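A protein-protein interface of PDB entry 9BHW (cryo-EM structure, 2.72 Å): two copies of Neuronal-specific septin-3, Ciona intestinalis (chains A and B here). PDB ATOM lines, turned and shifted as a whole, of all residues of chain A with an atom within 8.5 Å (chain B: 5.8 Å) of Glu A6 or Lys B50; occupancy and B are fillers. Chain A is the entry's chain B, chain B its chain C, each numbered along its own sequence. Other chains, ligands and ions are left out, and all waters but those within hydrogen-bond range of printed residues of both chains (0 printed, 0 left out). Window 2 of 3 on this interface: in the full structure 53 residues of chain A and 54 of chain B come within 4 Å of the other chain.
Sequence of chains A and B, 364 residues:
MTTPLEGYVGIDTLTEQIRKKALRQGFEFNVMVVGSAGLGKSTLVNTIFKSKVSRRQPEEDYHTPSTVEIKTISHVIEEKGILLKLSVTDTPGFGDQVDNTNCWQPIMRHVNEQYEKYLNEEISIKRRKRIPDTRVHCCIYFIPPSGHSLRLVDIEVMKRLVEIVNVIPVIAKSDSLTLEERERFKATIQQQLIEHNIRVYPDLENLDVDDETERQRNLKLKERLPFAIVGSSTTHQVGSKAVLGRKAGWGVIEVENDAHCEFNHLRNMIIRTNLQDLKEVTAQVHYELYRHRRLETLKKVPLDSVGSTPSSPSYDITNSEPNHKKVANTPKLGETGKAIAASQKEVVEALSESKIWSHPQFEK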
ATOM      1  N   THR A   3     -23.295  -5.704  12.279  1.00  0.00           N
ATOM      2  CA  THR A   3     -24.209  -6.826  12.427  1.00  0.00           C
ATOM      3  C   THR A   3     -23.472  -8.138  12.159  1.00  0.00           C
ATOM      4  O   THR A   3     -22.906  -8.321  11.078  1.00  0.00           O
ATOM      5  CB  THR A   3     -25.387  -6.686  11.469  1.00  0.00           C
ATOM      6  OG1 THR A   3     -25.980  -5.393  11.632  1.00  0.00           O
ATOM      7  CG2 THR A   3     -26.432  -7.728  11.775  1.00  0.00           C
ATOM      8  N   PRO A   4     -23.454  -9.055  13.125  1.00  0.00           N
ATOM      9  CA  PRO A   4     -22.687 -10.294  12.948  1.00  0.00           C
ATOM     10  C   PRO A   4     -23.265 -11.168  11.848  1.00  0.00           C
ATOM     11  O   PRO A   4     -24.472 -11.171  11.598  1.00  0.00           O
ATOM     12  CB  PRO A   4     -22.794 -10.973  14.317  1.00  0.00           C
ATOM     13  CG  PRO A   4     -24.042 -10.436  14.904  1.00  0.00           C
ATOM     14  CD  PRO A   4     -24.176  -9.028  14.407  1.00  0.00           C
ATOM     15  N   LEU A   5     -22.384 -11.917  11.189  1.00  0.00           N
ATOM     16  CA  LEU A   5     -22.776 -12.804  10.106  1.00  0.00           C
ATOM     17  C   LEU A   5     -22.802 -14.249  10.582  1.00  0.00           C
ATOM     18  O   LEU A   5     -22.000 -14.661  11.424  1.00  0.00           O
ATOM     19  CB  LEU A   5     -21.824 -12.668   8.921  1.00  0.00           C
ATOM     20  CG  LEU A   5     -21.913 -11.380   8.108  1.00  0.00           C
ATOM     21  CD1 LEU A   5     -21.090 -11.495   6.845  1.00  0.00           C
ATOM     22  CD2 LEU A   5     -23.352 -11.058   7.778  1.00  0.00           C
ATOM     23  N   GLU A   6     -23.740 -15.017  10.032  1.00  0.00           N
ATOM     24  CA  GLU A   6     -23.908 -16.424  10.370  1.00  0.00           C
ATOM     25  C   GLU A   6     -23.467 -17.345   9.241  1.00  0.00           C
ATOM     26  O   GLU A   6     -23.849 -18.519   9.217  1.00  0.00           O
ATOM     27  CB  GLU A   6     -25.363 -16.706  10.744  1.00  0.00           C
ATOM     28  CG  GLU A   6     -26.026 -15.594  11.535  1.00  0.00           C
ATOM     29  CD  GLU A   6     -27.528 -15.771  11.638  1.00  0.00           C
ATOM     30  OE1 GLU A   6     -28.166 -16.052  10.602  1.00  0.00           O
ATOM     31  OE2 GLU A   6     -28.069 -15.630  12.755  1.00  0.00           O
ATOM     32  N   GLY A   7     -22.677 -16.838   8.305  1.00  0.00           N
ATOM     33  CA  GLY A   7     -22.239 -17.647   7.188  1.00  0.00           C
ATOM     34  C   GLY A   7     -21.408 -16.820   6.234  1.00  0.00           C
ATOM     35  O   GLY A   7     -20.956 -15.722   6.565  1.00  0.00           O
ATOM     36  N   TYR A   8     -21.211 -17.364   5.040  1.00  0.00           N
ATOM     37  CA  TYR A   8     -20.436 -16.698   4.004  1.00  0.00           C
ATOM     38  C   TYR A   8     -21.388 -16.035   3.016  1.00  0.00           C
ATOM     39  O   TYR A   8     -22.277 -16.694   2.466  1.00  0.00           O
ATOM     40  CB  TYR A   8     -19.520 -17.696   3.300  1.00  0.00           C
ATOM     41  CG  TYR A   8     -18.627 -17.084   2.250  1.00  0.00           C
ATOM     42  CD1 TYR A   8     -17.837 -15.987   2.540  1.00  0.00           C
ATOM     43  CD2 TYR A   8     -18.568 -17.611   0.972  1.00  0.00           C
ATOM     44  CE1 TYR A   8     -17.021 -15.425   1.583  1.00  0.00           C
ATOM     45  CE2 TYR A   8     -17.755 -17.058   0.012  1.00  0.00           C
ATOM     46  CZ  TYR A   8     -16.985 -15.965   0.323  1.00  0.00           C
ATOM     47  OH  TYR A   8     -16.170 -15.411  -0.635  1.00  0.00           O
ATOM     48  N   VAL A   9     -21.202 -14.738   2.794  1.00  0.00           N
ATOM     49  CA  VAL A   9     -22.078 -13.953   1.932  1.00  0.00           C
ATOM     50  C   VAL A   9     -21.442 -13.687   0.575  1.00  0.00           C
ATOM     51  O   VAL A   9     -22.031 -13.986  -0.462  1.00  0.00           O
ATOM     52  CB  VAL A   9     -22.472 -12.635   2.633  1.00  0.00           C
ATOM     53  CG1 VAL A   9     -23.514 -11.899   1.820  1.00  0.00           C
ATOM     54  CG2 VAL A   9     -22.982 -12.921   4.022  1.00  0.00           C
ATOM     55  N   GLY A  10     -20.240 -13.120   0.558  1.00  0.00           N
ATOM     56  CA  GLY A  10     -19.542 -12.920  -0.694  1.00  0.00           C
ATOM     57  C   GLY A  10     -19.175 -11.485  -1.005  1.00  0.00           C
ATOM     58  O   GLY A  10     -18.863 -11.159  -2.152  1.00  0.00           O
ATOM     59  N   VAL B  45     -34.074 -11.419   2.178  1.00  0.00           N
ATOM     60  CA  VAL B  45     -32.999 -10.483   2.496  1.00  0.00           C
ATOM     61  C   VAL B  45     -32.135 -11.032   3.623  1.00  0.00           C
ATOM     62  O   VAL B  45     -30.909 -10.882   3.614  1.00  0.00           O
ATOM     63  CB  VAL B  45     -33.573  -9.097   2.833  1.00  0.00           C
ATOM     64  CG1 VAL B  45     -32.467  -8.158   3.265  1.00  0.00           C
ATOM     65  CG2 VAL B  45     -34.288  -8.531   1.628  1.00  0.00           C
ATOM     66  N   ASN B  46     -32.754 -11.692   4.603  1.00  0.00           N
ATOM     67  CA  ASN B  46     -31.979 -12.295   5.681  1.00  0.00           C
ATOM     68  C   ASN B  46     -31.111 -13.436   5.171  1.00  0.00           C
ATOM     69  O   ASN B  46     -30.009 -13.658   5.679  1.00  0.00           O
ATOM     70  CB  ASN B  46     -32.908 -12.789   6.784  1.00  0.00           C
ATOM     71  CG  ASN B  46     -33.378 -11.680   7.687  1.00  0.00           C
ATOM     72  OD1 ASN B  46     -32.896 -10.555   7.605  1.00  0.00           O
ATOM     73  ND2 ASN B  46     -34.322 -11.992   8.559  1.00  0.00           N
ATOM     74  N   THR B  47     -31.597 -14.179   4.177  1.00  0.00           N
ATOM     75  CA  THR B  47     -30.856 -15.321   3.653  1.00  0.00           C
ATOM     76  C   THR B  47     -29.710 -14.890   2.745  1.00  0.00           C
ATOM     77  O   THR B  47     -28.640 -15.507   2.763  1.00  0.00           O
ATOM     78  CB  THR B  47     -31.806 -16.253   2.903  1.00  0.00           C
ATOM     79  OG1 THR B  47     -32.895 -16.612   3.759  1.00  0.00           O
ATOM     80  CG2 THR B  47     -31.087 -17.512   2.471  1.00  0.00           C
ATOM     81  N   ILE B  48     -29.912 -13.839   1.947  1.00  0.00           N
ATOM     82  CA  ILE B  48     -28.861 -13.374   1.046  1.00  0.00           C
ATOM     83  C   ILE B  48     -27.638 -12.940   1.840  1.00  0.00           C
ATOM     84  O   ILE B  48     -26.504 -13.318   1.527  1.00  0.00           O
ATOM     85  CB  ILE B  48     -29.380 -12.234   0.155  1.00  0.00           C
ATOM     86  CG1 ILE B  48     -30.368 -12.757  -0.878  1.00  0.00           C
ATOM     87  CG2 ILE B  48     -28.236 -11.543  -0.548  1.00  0.00           C
ATOM     88  CD1 ILE B  48     -31.004 -11.670  -1.684  1.00  0.00           C
ATOM     89  N   PHE B  49     -27.850 -12.148   2.886  1.00  0.00           N
ATOM     90  CA  PHE B  49     -26.767 -11.630   3.703  1.00  0.00           C
ATOM     91  C   PHE B  49     -26.505 -12.471   4.941  1.00  0.00           C
ATOM     92  O   PHE B  49     -25.613 -12.133   5.723  1.00  0.00           O
ATOM     93  CB  PHE B  49     -27.060 -10.183   4.097  1.00  0.00           C
ATOM     94  CG  PHE B  49     -27.305  -9.284   2.925  1.00  0.00           C
ATOM     95  CD1 PHE B  49     -26.252  -8.759   2.208  1.00  0.00           C
ATOM     96  CD2 PHE B  49     -28.590  -8.979   2.528  1.00  0.00           C
ATOM     97  CE1 PHE B  49     -26.476  -7.944   1.127  1.00  0.00           C
ATOM     98  CE2 PHE B  49     -28.816  -8.162   1.446  1.00  0.00           C
ATOM     99  CZ  PHE B  49     -27.758  -7.646   0.747  1.00  0.00           C
ATOM    100  N   LYS B  50     -27.257 -13.555   5.131  1.00  0.00           N
ATOM    101  CA  LYS B  50     -27.032 -14.514   6.213  1.00  0.00           C
ATOM    102  C   LYS B  50     -26.899 -13.816   7.560  1.00  0.00           C
ATOM    103  O   LYS B  50     -26.040 -14.143   8.379  1.00  0.00           O
ATOM    104  CB  LYS B  50     -25.830 -15.403   5.913  1.00  0.00           C
ATOM    105  CG  LYS B  50     -26.086 -16.300   4.721  1.00  0.00           C
ATOM    106  CD  LYS B  50     -24.925 -17.202   4.406  1.00  0.00           C
ATOM    107  CE  LYS B  50     -25.287 -18.128   3.266  1.00  0.00           C
ATOM    108  NZ  LYS B  50     -25.476 -17.374   1.999  1.00  0.00           N
ATOM    109  N   SER B  51     -27.771 -12.841   7.783  1.00  0.00           N
ATOM    110  CA  SER B  51     -27.825 -12.114   9.038  1.00  0.00           C
ATOM    111  C   SER B  51     -29.201 -11.484   9.154  1.00  0.00           C
ATOM    112  O   SER B  51     -29.920 -11.333   8.164  1.00  0.00           O
ATOM    113  CB  SER B  51     -26.728 -11.054   9.119  1.00  0.00           C
ATOM    114  OG  SER B  51     -26.657 -10.509  10.420  1.00  0.00           O
ATOM    115  N   LYS B  52     -29.561 -11.117  10.382  1.00  0.00           N
ATOM    116  CA  LYS B  52     -30.856 -10.498  10.651  1.00  0.00           C
ATOM    117  C   LYS B  52     -30.788  -9.044  10.196  1.00  0.00           C
ATOM    118  O   LYS B  52     -30.586  -8.113  10.979  1.00  0.00           O
ATOM    119  CB  LYS B  52     -31.211 -10.629  12.123  1.00  0.00           C
ATOM    120  CG  LYS B  52     -31.536 -12.050  12.531  1.00  0.00           C
ATOM    121  CD  LYS B  52     -32.166 -12.106  13.905  1.00  0.00           C
ATOM    122  CE  LYS B  52     -32.633 -13.513  14.232  1.00  0.00           C
ATOM    123  NZ  LYS B  52     -33.192 -14.201  13.036  1.00  0.00           N
ATOM    124  N   SER B 233     -34.011 -19.275   7.181  1.00  0.00           N
ATOM    125  CA  SER B 233     -32.978 -18.930   8.144  1.00  0.00           C
ATOM    126  C   SER B 233     -32.818 -19.968   9.243  1.00  0.00           C
ATOM    127  O   SER B 233     -32.028 -19.745  10.165  1.00  0.00           O
ATOM    128  CB  SER B 233     -33.268 -17.563   8.777  1.00  0.00           C
ATOM    129  OG  SER B 233     -32.097 -17.009   9.347  1.00  0.00           O
ATOM    130  N   LEU B 244     -29.234 -24.815   5.602  1.00  0.00           N
ATOM    131  CA  LEU B 244     -30.341 -23.872   5.628  1.00  0.00           C
ATOM    132  C   LEU B 244     -31.483 -24.394   4.774  1.00  0.00           C
ATOM    133  O   LEU B 244     -31.274 -24.860   3.652  1.00  0.00           O
ATOM    134  CB  LEU B 244     -29.908 -22.502   5.112  1.00  0.00           C
ATOM    135  CG  LEU B 244     -29.102 -21.564   6.004  1.00  0.00           C
ATOM    136  CD1 LEU B 244     -27.678 -22.066   6.191  1.00  0.00           C
ATOM    137  CD2 LEU B 244     -29.106 -20.174   5.408  1.00  0.00           C
ATOM    138  N   GLU B 256     -29.670 -23.643  -0.468  1.00  0.00           N
ATOM    139  CA  GLU B 256     -28.400 -23.590  -1.177  1.00  0.00           C
ATOM    140  C   GLU B 256     -28.271 -24.653  -2.261  1.00  0.00           C
ATOM    141  O   GLU B 256     -27.249 -24.684  -2.951  1.00  0.00           O
ATOM    142  CB  GLU B 256     -27.248 -23.734  -0.182  1.00  0.00           C
ATOM    143  CG  GLU B 256     -27.115 -22.581   0.799  1.00  0.00           C
ATOM    144  CD  GLU B 256     -26.719 -21.284   0.131  1.00  0.00           C
ATOM    145  OE1 GLU B 256     -25.992 -21.332  -0.882  1.00  0.00           O
ATOM    146  OE2 GLU B 256     -27.132 -20.213   0.623  1.00  0.00           O
ATOM    147  N   PHE B 263     -31.956 -19.877  -5.793  1.00  0.00           N
ATOM    148  CA  PHE B 263     -31.487 -18.816  -4.909  1.00  0.00           C
ATOM    149  C   PHE B 263     -30.013 -18.522  -5.137  1.00  0.00           C
ATOM    150  O   PHE B 263     -29.576 -17.370  -5.018  1.00  0.00           O
ATOM    151  CB  PHE B 263     -31.724 -19.204  -3.454  1.00  0.00           C
ATOM    152  CG  PHE B 263     -30.990 -18.347  -2.471  1.00  0.00           C
ATOM    153  CD1 PHE B 263     -31.487 -17.113  -2.109  1.00  0.00           C
ATOM    154  CD2 PHE B 263     -29.808 -18.775  -1.903  1.00  0.00           C
ATOM    155  CE1 PHE B 263     -30.817 -16.329  -1.207  1.00  0.00           C
ATOM    156  CE2 PHE B 263     -29.139 -17.991  -0.997  1.00  0.00           C
ATOM    157  CZ  PHE B 263     -29.642 -16.768  -0.652  1.00  0.00           C
ATOM    158  N   ARG B 267     -28.240 -14.835  -5.608  1.00  0.00           N
ATOM    159  CA  ARG B 267     -27.249 -14.329  -4.666  1.00  0.00           C
ATOM    160  C   ARG B 267     -25.897 -14.118  -5.336  1.00  0.00           C
ATOM    161  O   ARG B 267     -25.191 -13.155  -5.018  1.00  0.00           O
ATOM    162  CB  ARG B 267     -27.148 -15.270  -3.470  1.00  0.00           C
ATOM    163  CG  ARG B 267     -26.194 -14.828  -2.387  1.00  0.00           C
ATOM    164  CD  ARG B 267     -26.211 -15.834  -1.251  1.00  0.00           C
ATOM    165  NE  ARG B 267     -25.747 -17.152  -1.659  1.00  0.00           N
ATOM    166  CZ  ARG B 267     -24.473 -17.498  -1.726  1.00  0.00           C
ATOM    167  NH1 ARG B 267     -23.517 -16.663  -1.363  1.00  0.00           N
ATOM    168  NH2 ARG B 267     -24.152 -18.713  -2.153  1.00  0.00           N
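OD1 of Asn B46 sits close to O of Ser B51.
The side-chain amino group (NZ) of Lys B50 lies within salt-bridge range of the side-chain carboxylate (OE2) of Glu B256, at 3.6 Å.
NH2 of Arg B267 is in salt-bridge range of OE1 of Glu B256.
Of the 8 printed residues of chain A, 7 touch a printed residue of chain B.
No position is printed for both chains.
Of the 11 pairs that touch across the chains among the printed residues, none has its exchanged pair printed and touching as well.
The side-chain hydroxyl (OG) of Ser B51 is in hydrogen-bond range of the backbone carbonyl oxygen (O) of Pro A4 (2.6 Å).
The backbone carbonyl oxygen of Lys B50 lies within hydrogen-bond range of the backbone NH of Glu A6 (3.0 Å).
O of Tyr A8 lies within hydrogen-bond range of NZ of Lys B50 (3.3 Å).
The backbone carbonyl oxygen of Val A9 lies within hydrogen-bond range of the guanidinium group of Arg B267, 3.2 Å away.
Ser B51 touches Thr A3.
Leu A5 touches Phe B49 (CD2 to O, 3.2 Å).
C of Leu A5 touches O of Lys B50 (3.9 Å).
Ser B51 touches Leu A5 (CB to CD2, 3.6 Å).
Gly A7 touches Lys B50.
Val A9 touches Ile B48.
Val A9 touches Phe B49 (CG2 to O, 3.2 Å).
Of chain B, only Lys B50 comes within 4 Å of Glu A6.
Of the printed residues of chain B, Tyr A8 touches Lys B50.
Printed residues of chain A within 4 Å of Ile B48: Val A9.
Of chain A, only Leu A5 (3.9 Å), Glu A6 (3.0 Å), Gly A7 (3.9 Å) and Tyr A8 (3.3 Å) come within 4 Å of Lys B50.
Of chain A, only Thr A3 (3.1 Å), Pro A4 (2.6 Å) and Leu A5 (3.6 Å) come within 4 Å of Ser B51.
The nearest printed residue of chain B that does not touch Glu A6 is Ser B233 (4.2 Å).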
